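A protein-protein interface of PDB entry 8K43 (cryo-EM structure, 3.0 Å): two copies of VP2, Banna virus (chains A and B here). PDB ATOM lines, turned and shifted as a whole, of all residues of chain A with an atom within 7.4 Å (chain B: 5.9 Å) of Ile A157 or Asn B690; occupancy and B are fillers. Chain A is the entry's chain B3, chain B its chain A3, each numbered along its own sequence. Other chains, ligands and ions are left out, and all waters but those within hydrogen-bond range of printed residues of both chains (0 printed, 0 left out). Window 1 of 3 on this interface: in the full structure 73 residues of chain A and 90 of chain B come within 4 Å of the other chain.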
ATOM      1  N   GLY A 148     -21.388   4.194 -27.488  1.00  0.00           N
ATOM      2  CA  GLY A 148     -20.263   3.841 -26.652  1.00  0.00           C
ATOM      3  C   GLY A 148     -19.207   3.048 -27.393  1.00  0.00           C
ATOM      4  O   GLY A 148     -19.464   2.454 -28.438  1.00  0.00           O
ATOM      5  N   VAL A 149     -17.998   3.042 -26.829  1.00  0.00           N
ATOM      6  CA  VAL A 149     -16.894   2.321 -27.445  1.00  0.00           C
ATOM      7  C   VAL A 149     -17.178   0.826 -27.406  1.00  0.00           C
ATOM      8  O   VAL A 149     -17.742   0.304 -26.435  1.00  0.00           O
ATOM      9  CB  VAL A 149     -15.569   2.670 -26.748  1.00  0.00           C
ATOM     10  CG1 VAL A 149     -15.257   4.143 -26.934  1.00  0.00           C
ATOM     11  CG2 VAL A 149     -15.638   2.344 -25.275  1.00  0.00           C
ATOM     12  N   THR A 150     -16.817   0.133 -28.480  1.00  0.00           N
ATOM     13  CA  THR A 150     -17.140  -1.274 -28.662  1.00  0.00           C
ATOM     14  C   THR A 150     -15.886  -2.128 -28.526  1.00  0.00           C
ATOM     15  O   THR A 150     -14.780  -1.629 -28.301  1.00  0.00           O
ATOM     16  CB  THR A 150     -17.805  -1.498 -30.021  1.00  0.00           C
ATOM     17  OG1 THR A 150     -16.800  -1.570 -31.038  1.00  0.00           O
ATOM     18  CG2 THR A 150     -18.759  -0.360 -30.340  1.00  0.00           C
ATOM     19  N   SER A 151     -16.073  -3.443 -28.663  1.00  0.00           N
ATOM     20  CA  SER A 151     -14.951  -4.365 -28.543  1.00  0.00           C
ATOM     21  C   SER A 151     -14.013  -4.270 -29.737  1.00  0.00           C
ATOM     22  O   SER A 151     -12.809  -4.508 -29.597  1.00  0.00           O
ATOM     23  CB  SER A 151     -15.458  -5.795 -28.388  1.00  0.00           C
ATOM     24  OG  SER A 151     -15.641  -6.408 -29.650  1.00  0.00           O
ATOM     25  N   GLU A 152     -14.541  -3.939 -30.916  1.00  0.00           N
ATOM     26  CA  GLU A 152     -13.688  -3.789 -32.089  1.00  0.00           C
ATOM     27  C   GLU A 152     -12.695  -2.651 -31.904  1.00  0.00           C
ATOM     28  O   GLU A 152     -11.523  -2.774 -32.280  1.00  0.00           O
ATOM     29  CB  GLU A 152     -14.542  -3.564 -33.335  1.00  0.00           C
ATOM     30  CG  GLU A 152     -15.693  -4.542 -33.479  1.00  0.00           C
ATOM     31  CD  GLU A 152     -15.236  -5.916 -33.928  1.00  0.00           C
ATOM     32  OE1 GLU A 152     -14.902  -6.747 -33.057  1.00  0.00           O
ATOM     33  OE2 GLU A 152     -15.210  -6.164 -35.151  1.00  0.00           O
ATOM     34  N   ASP A 153     -13.144  -1.533 -31.330  1.00  0.00           N
ATOM     35  CA  ASP A 153     -12.228  -0.436 -31.045  1.00  0.00           C
ATOM     36  C   ASP A 153     -11.190  -0.840 -30.007  1.00  0.00           C
ATOM     37  O   ASP A 153     -10.012  -0.483 -30.124  1.00  0.00           O
ATOM     38  CB  ASP A 153     -13.004   0.793 -30.573  1.00  0.00           C
ATOM     39  CG  ASP A 153     -14.336   0.946 -31.277  1.00  0.00           C
ATOM     40  OD1 ASP A 153     -14.343   1.363 -32.456  1.00  0.00           O
ATOM     41  OD2 ASP A 153     -15.377   0.655 -30.653  1.00  0.00           O
ATOM     42  N   MET A 154     -11.609  -1.581 -28.980  1.00  0.00           N
ATOM     43  CA  MET A 154     -10.668  -2.025 -27.958  1.00  0.00           C
ATOM     44  C   MET A 154      -9.639  -2.984 -28.539  1.00  0.00           C
ATOM     45  O   MET A 154      -8.461  -2.944 -28.164  1.00  0.00           O
ATOM     46  CB  MET A 154     -11.419  -2.679 -26.799  1.00  0.00           C
ATOM     47  CG  MET A 154     -11.906  -1.699 -25.744  1.00  0.00           C
ATOM     48  SD  MET A 154     -10.862  -0.238 -25.615  1.00  0.00           S
ATOM     49  CE  MET A 154      -9.948  -0.604 -24.121  1.00  0.00           C
ATOM     50  N   ALA A 155     -10.065  -3.860 -29.450  1.00  0.00           N
ATOM     51  CA  ALA A 155      -9.131  -4.781 -30.087  1.00  0.00           C
ATOM     52  C   ALA A 155      -8.087  -4.031 -30.904  1.00  0.00           C
ATOM     53  O   ALA A 155      -6.908  -4.397 -30.903  1.00  0.00           O
ATOM     54  CB  ALA A 155      -9.889  -5.773 -30.968  1.00  0.00           C
ATOM     55  N   LYS A 156      -8.507  -2.983 -31.615  1.00  0.00           N
ATOM     56  CA  LYS A 156      -7.560  -2.187 -32.387  1.00  0.00           C
ATOM     57  C   LYS A 156      -6.602  -1.427 -31.479  1.00  0.00           C
ATOM     58  O   LYS A 156      -5.399  -1.355 -31.757  1.00  0.00           O
ATOM     59  CB  LYS A 156      -8.311  -1.219 -33.296  1.00  0.00           C
ATOM     60  CG  LYS A 156      -8.932  -1.872 -34.512  1.00  0.00           C
ATOM     61  CD  LYS A 156      -8.957  -0.926 -35.693  1.00  0.00           C
ATOM     62  CE  LYS A 156      -7.706  -1.076 -36.539  1.00  0.00           C
ATOM     63  NZ  LYS A 156      -7.585  -2.447 -37.101  1.00  0.00           N
ATOM     64  N   ILE A 157      -7.115  -0.846 -30.394  1.00  0.00           N
ATOM     65  CA  ILE A 157      -6.276  -0.045 -29.507  1.00  0.00           C
ATOM     66  C   ILE A 157      -5.215  -0.914 -28.847  1.00  0.00           C
ATOM     67  O   ILE A 157      -4.043  -0.535 -28.765  1.00  0.00           O
ATOM     68  CB  ILE A 157      -7.142   0.682 -28.464  1.00  0.00           C
ATOM     69  CG1 ILE A 157      -7.893   1.841 -29.112  1.00  0.00           C
ATOM     70  CG2 ILE A 157      -6.286   1.186 -27.317  1.00  0.00           C
ATOM     71  CD1 ILE A 157      -9.056   2.336 -28.296  1.00  0.00           C
ATOM     72  N   TYR A 158      -5.610  -2.094 -28.366  1.00  0.00           N
ATOM     73  CA  TYR A 158      -4.657  -2.980 -27.712  1.00  0.00           C
ATOM     74  C   TYR A 158      -3.614  -3.493 -28.695  1.00  0.00           C
ATOM     75  O   TYR A 158      -2.442  -3.650 -28.337  1.00  0.00           O
ATOM     76  CB  TYR A 158      -5.394  -4.138 -27.048  1.00  0.00           C
ATOM     77  CG  TYR A 158      -6.118  -3.745 -25.782  1.00  0.00           C
ATOM     78  CD1 TYR A 158      -5.754  -2.607 -25.080  1.00  0.00           C
ATOM     79  CD2 TYR A 158      -7.162  -4.512 -25.289  1.00  0.00           C
ATOM     80  CE1 TYR A 158      -6.409  -2.247 -23.923  1.00  0.00           C
ATOM     81  CE2 TYR A 158      -7.820  -4.158 -24.134  1.00  0.00           C
ATOM     82  CZ  TYR A 158      -7.441  -3.027 -23.456  1.00  0.00           C
ATOM     83  OH  TYR A 158      -8.100  -2.672 -22.303  1.00  0.00           O
ATOM     84  N   GLY A 159      -4.022  -3.770 -29.932  1.00  0.00           N
ATOM     85  CA  GLY A 159      -3.061  -4.195 -30.936  1.00  0.00           C
ATOM     86  C   GLY A 159      -2.052  -3.113 -31.268  1.00  0.00           C
ATOM     87  O   GLY A 159      -0.870  -3.396 -31.477  1.00  0.00           O
ATOM     88  N   ALA A 160      -2.507  -1.860 -31.330  1.00  0.00           N
ATOM     89  CA  ALA A 160      -1.590  -0.753 -31.577  1.00  0.00           C
ATOM     90  C   ALA A 160      -0.577  -0.614 -30.450  1.00  0.00           C
ATOM     91  O   ALA A 160       0.610  -0.375 -30.697  1.00  0.00           O
ATOM     92  CB  ALA A 160      -2.373   0.546 -31.757  1.00  0.00           C
ATOM     93  N   VAL A 161      -1.030  -0.752 -29.202  1.00  0.00           N
ATOM     94  CA  VAL A 161      -0.115  -0.685 -28.066  1.00  0.00           C
ATOM     95  C   VAL A 161       0.861  -1.850 -28.101  1.00  0.00           C
ATOM     96  O   VAL A 161       2.053  -1.689 -27.811  1.00  0.00           O
ATOM     97  CB  VAL A 161      -0.906  -0.645 -26.746  1.00  0.00           C
ATOM     98  CG1 VAL A 161       0.038  -0.683 -25.560  1.00  0.00           C
ATOM     99  CG2 VAL A 161      -1.777   0.595 -26.693  1.00  0.00           C
ATOM    100  N   ALA A 162       0.377  -3.042 -28.454  1.00  0.00           N
ATOM    101  CA  ALA A 162       1.251  -4.207 -28.519  1.00  0.00           C
ATOM    102  C   ALA A 162       2.310  -4.045 -29.601  1.00  0.00           C
ATOM    103  O   ALA A 162       3.424  -4.563 -29.472  1.00  0.00           O
ATOM    104  CB  ALA A 162       0.427  -5.471 -28.758  1.00  0.00           C
ATOM    105  N   ALA A 163       1.976  -3.340 -30.685  1.00  0.00           N
ATOM    106  CA  ALA A 163       2.951  -3.103 -31.743  1.00  0.00           C
ATOM    107  C   ALA A 163       4.107  -2.241 -31.252  1.00  0.00           C
ATOM    108  O   ALA A 163       5.267  -2.493 -31.595  1.00  0.00           O
ATOM    109  CB  ALA A 163       2.272  -2.454 -32.947  1.00  0.00           C
ATOM    110  N   ALA B 685     -17.798  11.966 -30.752  1.00  0.00           N
ATOM    111  CA  ALA B 685     -17.479  11.803 -29.338  1.00  0.00           C
ATOM    112  C   ALA B 685     -16.809  10.460 -29.080  1.00  0.00           C
ATOM    113  O   ALA B 685     -15.837  10.373 -28.323  1.00  0.00           O
ATOM    114  CB  ALA B 685     -18.744  11.945 -28.496  1.00  0.00           C
ATOM    115  N   ARG B 686     -17.326   9.398 -29.700  1.00  0.00           N
ATOM    116  CA  ARG B 686     -16.708   8.086 -29.556  1.00  0.00           C
ATOM    117  C   ARG B 686     -15.311   8.069 -30.153  1.00  0.00           C
ATOM    118  O   ARG B 686     -14.397   7.446 -29.602  1.00  0.00           O
ATOM    119  CB  ARG B 686     -17.580   7.022 -30.220  1.00  0.00           C
ATOM    120  CG  ARG B 686     -17.477   5.659 -29.575  1.00  0.00           C
ATOM    121  CD  ARG B 686     -18.150   4.611 -30.432  1.00  0.00           C
ATOM    122  NE  ARG B 686     -17.694   4.674 -31.812  1.00  0.00           N
ATOM    123  CZ  ARG B 686     -18.376   4.200 -32.845  1.00  0.00           C
ATOM    124  NH1 ARG B 686     -19.555   3.621 -32.686  1.00  0.00           N
ATOM    125  NH2 ARG B 686     -17.865   4.312 -34.067  1.00  0.00           N
ATOM    126  N   ASP B 687     -15.129   8.750 -31.283  1.00  0.00           N
ATOM    127  CA  ASP B 687     -13.827   8.769 -31.937  1.00  0.00           C
ATOM    128  C   ASP B 687     -12.795   9.511 -31.097  1.00  0.00           C
ATOM    129  O   ASP B 687     -11.620   9.125 -31.061  1.00  0.00           O
ATOM    130  CB  ASP B 687     -13.961   9.397 -33.320  1.00  0.00           C
ATOM    131  CG  ASP B 687     -14.179   8.365 -34.408  1.00  0.00           C
ATOM    132  OD1 ASP B 687     -14.048   7.157 -34.114  1.00  0.00           O
ATOM    133  OD2 ASP B 687     -14.479   8.759 -35.553  1.00  0.00           O
ATOM    134  N   ILE B 688     -13.210  10.580 -30.416  1.00  0.00           N
ATOM    135  CA  ILE B 688     -12.294  11.298 -29.534  1.00  0.00           C
ATOM    136  C   ILE B 688     -11.952  10.449 -28.318  1.00  0.00           C
ATOM    137  O   ILE B 688     -10.792  10.392 -27.889  1.00  0.00           O
ATOM    138  CB  ILE B 688     -12.896  12.655 -29.125  1.00  0.00           C
ATOM    139  CG1 ILE B 688     -13.023  13.569 -30.341  1.00  0.00           C
ATOM    140  CG2 ILE B 688     -12.044  13.318 -28.065  1.00  0.00           C
ATOM    141  CD1 ILE B 688     -14.061  14.650 -30.175  1.00  0.00           C
ATOM    142  N   SER B 689     -12.952   9.777 -27.741  1.00  0.00           N
ATOM    143  CA  SER B 689     -12.703   8.946 -26.569  1.00  0.00           C
ATOM    144  C   SER B 689     -11.752   7.803 -26.895  1.00  0.00           C
ATOM    145  O   SER B 689     -10.870   7.470 -26.094  1.00  0.00           O
ATOM    146  CB  SER B 689     -14.020   8.404 -26.019  1.00  0.00           C
ATOM    147  OG  SER B 689     -13.788   7.430 -25.017  1.00  0.00           O
ATOM    148  N   ASN B 690     -11.918   7.184 -28.064  1.00  0.00           N
ATOM    149  CA  ASN B 690     -10.972   6.163 -28.500  1.00  0.00           C
ATOM    150  C   ASN B 690      -9.581   6.750 -28.688  1.00  0.00           C
ATOM    151  O   ASN B 690      -8.582   6.150 -28.276  1.00  0.00           O
ATOM    152  CB  ASN B 690     -11.457   5.519 -29.796  1.00  0.00           C
ATOM    153  CG  ASN B 690     -12.568   4.520 -29.570  1.00  0.00           C
ATOM    154  OD1 ASN B 690     -12.521   3.724 -28.635  1.00  0.00           O
ATOM    155  ND2 ASN B 690     -13.579   4.559 -30.428  1.00  0.00           N
ATOM    156  N   SER B 691      -9.497   7.925 -29.313  1.00  0.00           N
ATOM    157  CA  SER B 691      -8.202   8.537 -29.582  1.00  0.00           C
ATOM    158  C   SER B 691      -7.488   8.916 -28.292  1.00  0.00           C
ATOM    159  O   SER B 691      -6.272   8.731 -28.169  1.00  0.00           O
ATOM    160  CB  SER B 691      -8.385   9.763 -30.474  1.00  0.00           C
ATOM    161  OG  SER B 691      -7.145  10.203 -30.992  1.00  0.00           O
ATOM    162  N   LEU B 692      -8.227   9.453 -27.320  1.00  0.00           N
ATOM    163  CA  LEU B 692      -7.620   9.829 -26.047  1.00  0.00           C
ATOM    164  C   LEU B 692      -7.077   8.613 -25.311  1.00  0.00           C
ATOM    165  O   LEU B 692      -5.994   8.670 -24.716  1.00  0.00           O
ATOM    166  CB  LEU B 692      -8.639  10.572 -25.184  1.00  0.00           C
ATOM    167  CG  LEU B 692      -8.962  12.004 -25.613  1.00  0.00           C
ATOM    168  CD1 LEU B 692     -10.019  12.613 -24.715  1.00  0.00           C
ATOM    169  CD2 LEU B 692      -7.707  12.847 -25.597  1.00  0.00           C
ATOM    170  N   THR B 693      -7.819   7.503 -25.328  1.00  0.00           N
ATOM    171  CA  THR B 693      -7.360   6.292 -24.653  1.00  0.00           C
ATOM    172  C   THR B 693      -6.104   5.734 -25.310  1.00  0.00           C
ATOM    173  O   THR B 693      -5.180   5.287 -24.621  1.00  0.00           O
ATOM    174  CB  THR B 693      -8.471   5.243 -24.647  1.00  0.00           C
ATOM    175  OG1 THR B 693      -9.625   5.771 -23.983  1.00  0.00           O
ATOM    176  CG2 THR B 693      -8.014   3.988 -23.928  1.00  0.00           C
ATOM    177  N   LEU B 694      -6.053   5.753 -26.641  1.00  0.00           N
ATOM    178  CA  LEU B 694      -4.888   5.239 -27.352  1.00  0.00           C
ATOM    179  C   LEU B 694      -3.637   6.042 -27.021  1.00  0.00           C
ATOM    180  O   LEU B 694      -2.556   5.474 -26.839  1.00  0.00           O
ATOM    181  CB  LEU B 694      -5.153   5.255 -28.855  1.00  0.00           C
ATOM    182  CG  LEU B 694      -4.017   4.851 -29.789  1.00  0.00           C
ATOM    183  CD1 LEU B 694      -3.430   3.516 -29.371  1.00  0.00           C
ATOM    184  CD2 LEU B 694      -4.521   4.791 -31.214  1.00  0.00           C
ATOM    185  N   VAL B 695      -3.771   7.366 -26.936  1.00  0.00           N
ATOM    186  CA  VAL B 695      -2.616   8.226 -26.699  1.00  0.00           C
ATOM    187  C   VAL B 695      -1.992   7.931 -25.341  1.00  0.00           C
ATOM    188  O   VAL B 695      -0.763   7.895 -25.201  1.00  0.00           O
ATOM    189  CB  VAL B 695      -3.026   9.705 -26.827  1.00  0.00           C
ATOM    190  CG1 VAL B 695      -2.086  10.598 -26.037  1.00  0.00           C
ATOM    191  CG2 VAL B 695      -3.059  10.119 -28.286  1.00  0.00           C
ATOM    192  N   HIS B 722      -1.180   0.845 -37.923  1.00  0.00           N
ATOM    193  CA  HIS B 722      -2.044  -0.209 -37.407  1.00  0.00           C
ATOM    194  C   HIS B 722      -3.499   0.237 -37.355  1.00  0.00           C
ATOM    195  O   HIS B 722      -4.402  -0.545 -37.671  1.00  0.00           O
ATOM    196  CB  HIS B 722      -1.570  -0.644 -36.023  1.00  0.00           C
ATOM    197  CG  HIS B 722      -2.278  -1.851 -35.496  1.00  0.00           C
ATOM    198  ND1 HIS B 722      -1.948  -3.133 -35.881  1.00  0.00           N
ATOM    199  CD2 HIS B 722      -3.299  -1.973 -34.616  1.00  0.00           C
ATOM    200  CE1 HIS B 722      -2.737  -3.992 -35.260  1.00  0.00           C
ATOM    201  NE2 HIS B 722      -3.564  -3.314 -34.486  1.00  0.00           N
ATOM    202  N   LEU B 729      -9.856   2.634 -37.179  1.00  0.00           N
ATOM    203  CA  LEU B 729     -10.399   2.871 -35.846  1.00  0.00           C
ATOM    204  C   LEU B 729     -11.269   4.119 -35.807  1.00  0.00           C
ATOM    205  O   LEU B 729     -12.186   4.208 -34.983  1.00  0.00           O
ATOM    206  CB  LEU B 729      -9.257   2.984 -34.835  1.00  0.00           C
ATOM    207  CG  LEU B 729      -9.603   3.343 -33.391  1.00  0.00           C
ATOM    208  CD1 LEU B 729     -10.027   2.109 -32.617  1.00  0.00           C
ATOM    209  CD2 LEU B 729      -8.427   4.022 -32.720  1.00  0.00           C
ATOM    210  N   TYR B 749      -4.594  12.524 -39.079  1.00  0.00           N
ATOM    211  CA  TYR B 749      -4.736  11.903 -37.768  1.00  0.00           C
ATOM    212  C   TYR B 749      -3.414  11.886 -37.017  1.00  0.00           C
ATOM    213  O   TYR B 749      -3.387  12.060 -35.794  1.00  0.00           O
ATOM    214  CB  TYR B 749      -5.288  10.488 -37.921  1.00  0.00           C
ATOM    215  CG  TYR B 749      -5.842   9.903 -36.645  1.00  0.00           C
ATOM    216  CD1 TYR B 749      -6.903  10.502 -35.988  1.00  0.00           C
ATOM    217  CD2 TYR B 749      -5.312   8.742 -36.105  1.00  0.00           C
ATOM    218  CE1 TYR B 749      -7.411   9.970 -34.823  1.00  0.00           C
ATOM    219  CE2 TYR B 749      -5.815   8.202 -34.945  1.00  0.00           C
ATOM    220  CZ  TYR B 749      -6.865   8.818 -34.309  1.00  0.00           C
ATOM    221  OH  TYR B 749      -7.369   8.280 -33.149  1.00  0.00           O
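N of Thr A150 lies within hydrogen-bond range of OD2 of Asp A153, at 2.7 Å.
O of Arg B686 sits at hydrogen-bond distance from ND2 of Asn B690 (3.1 Å).
Among the printed residues, merely in contact across the chains: Gly A148 with Arg B686 (3.2 Å), Val A149 with Arg B686 (3.8 Å), Val A149 with Asn B690 (3.2 Å), Asp A153 with Asn B690 (3.5 Å), Asp A153 with Leu B729 (3.6 Å), Lys A156 with His B722 (3.5 Å), Lys A156 with Leu B729 (3.8 Å), Ile A157 with Asn B690 (3.7 Å), Gly A159 with His B722 (3.6 Å), Ala A160 with Leu B694 (3.95 Å) and Ala A160 with His B722 (3.4 Å).
Of the printed residues of chain B, Asp A153 touches Asn B690 and Leu B729.
Ala A155 touches none of the printed residues of chain B.
Ile A157 touches just one residue of chain B: Asn B690 (3.7 Å).
Tyr A158 touches none of the printed residues of chain B.
Of the printed residues of chain B, Gly A159 touches His B722 (3.6 Å).
Of chain A, only Val A149 (3.2 Å), Asp A153 (3.5 Å) and Ile A157 (3.7 Å) come within 4 Å of Asn B690.
The nearest printed residue of chain B that does not touch Ile A157 is Leu B729 (4.1 Å).
The nearest residue of chain A that does not touch Asn B690 is Met A154 (5.3 Å).
The nearest printed residue of chain A that does not touch Leu B694 is Ile A157 (4.1 Å).
Hydrophobic or aromatic side chains of chain B that line the printed part of chain A: Leu B694, His B722 and Leu B729.
Of the 16 printed residues of chain A, 7 touch a printed residue of chain B.
Printed residues of chain A that touch a printed residue of chain B: Gly A148, Val A149, Asp A153, Lys A156, Ile A157, Gly A159 and Ala A160.
Hydrophobic or aromatic side chains of chain A within 4 Å of the printed part of chain B: Val A149, Ile A157 and Ala A160.
Along chain A the printed residues that touch a printed residue of chain B span positions 148 to 160.
Among the printed residues, no Asp or Glu carboxylate lies within 4 Å of a Lys or Arg side-chain nitrogen of the other chain.
No position is printed for both chains.
Of the 11 pairs that touch across the chains among the printed residues, none has its exchanged pair printed and touching as well.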
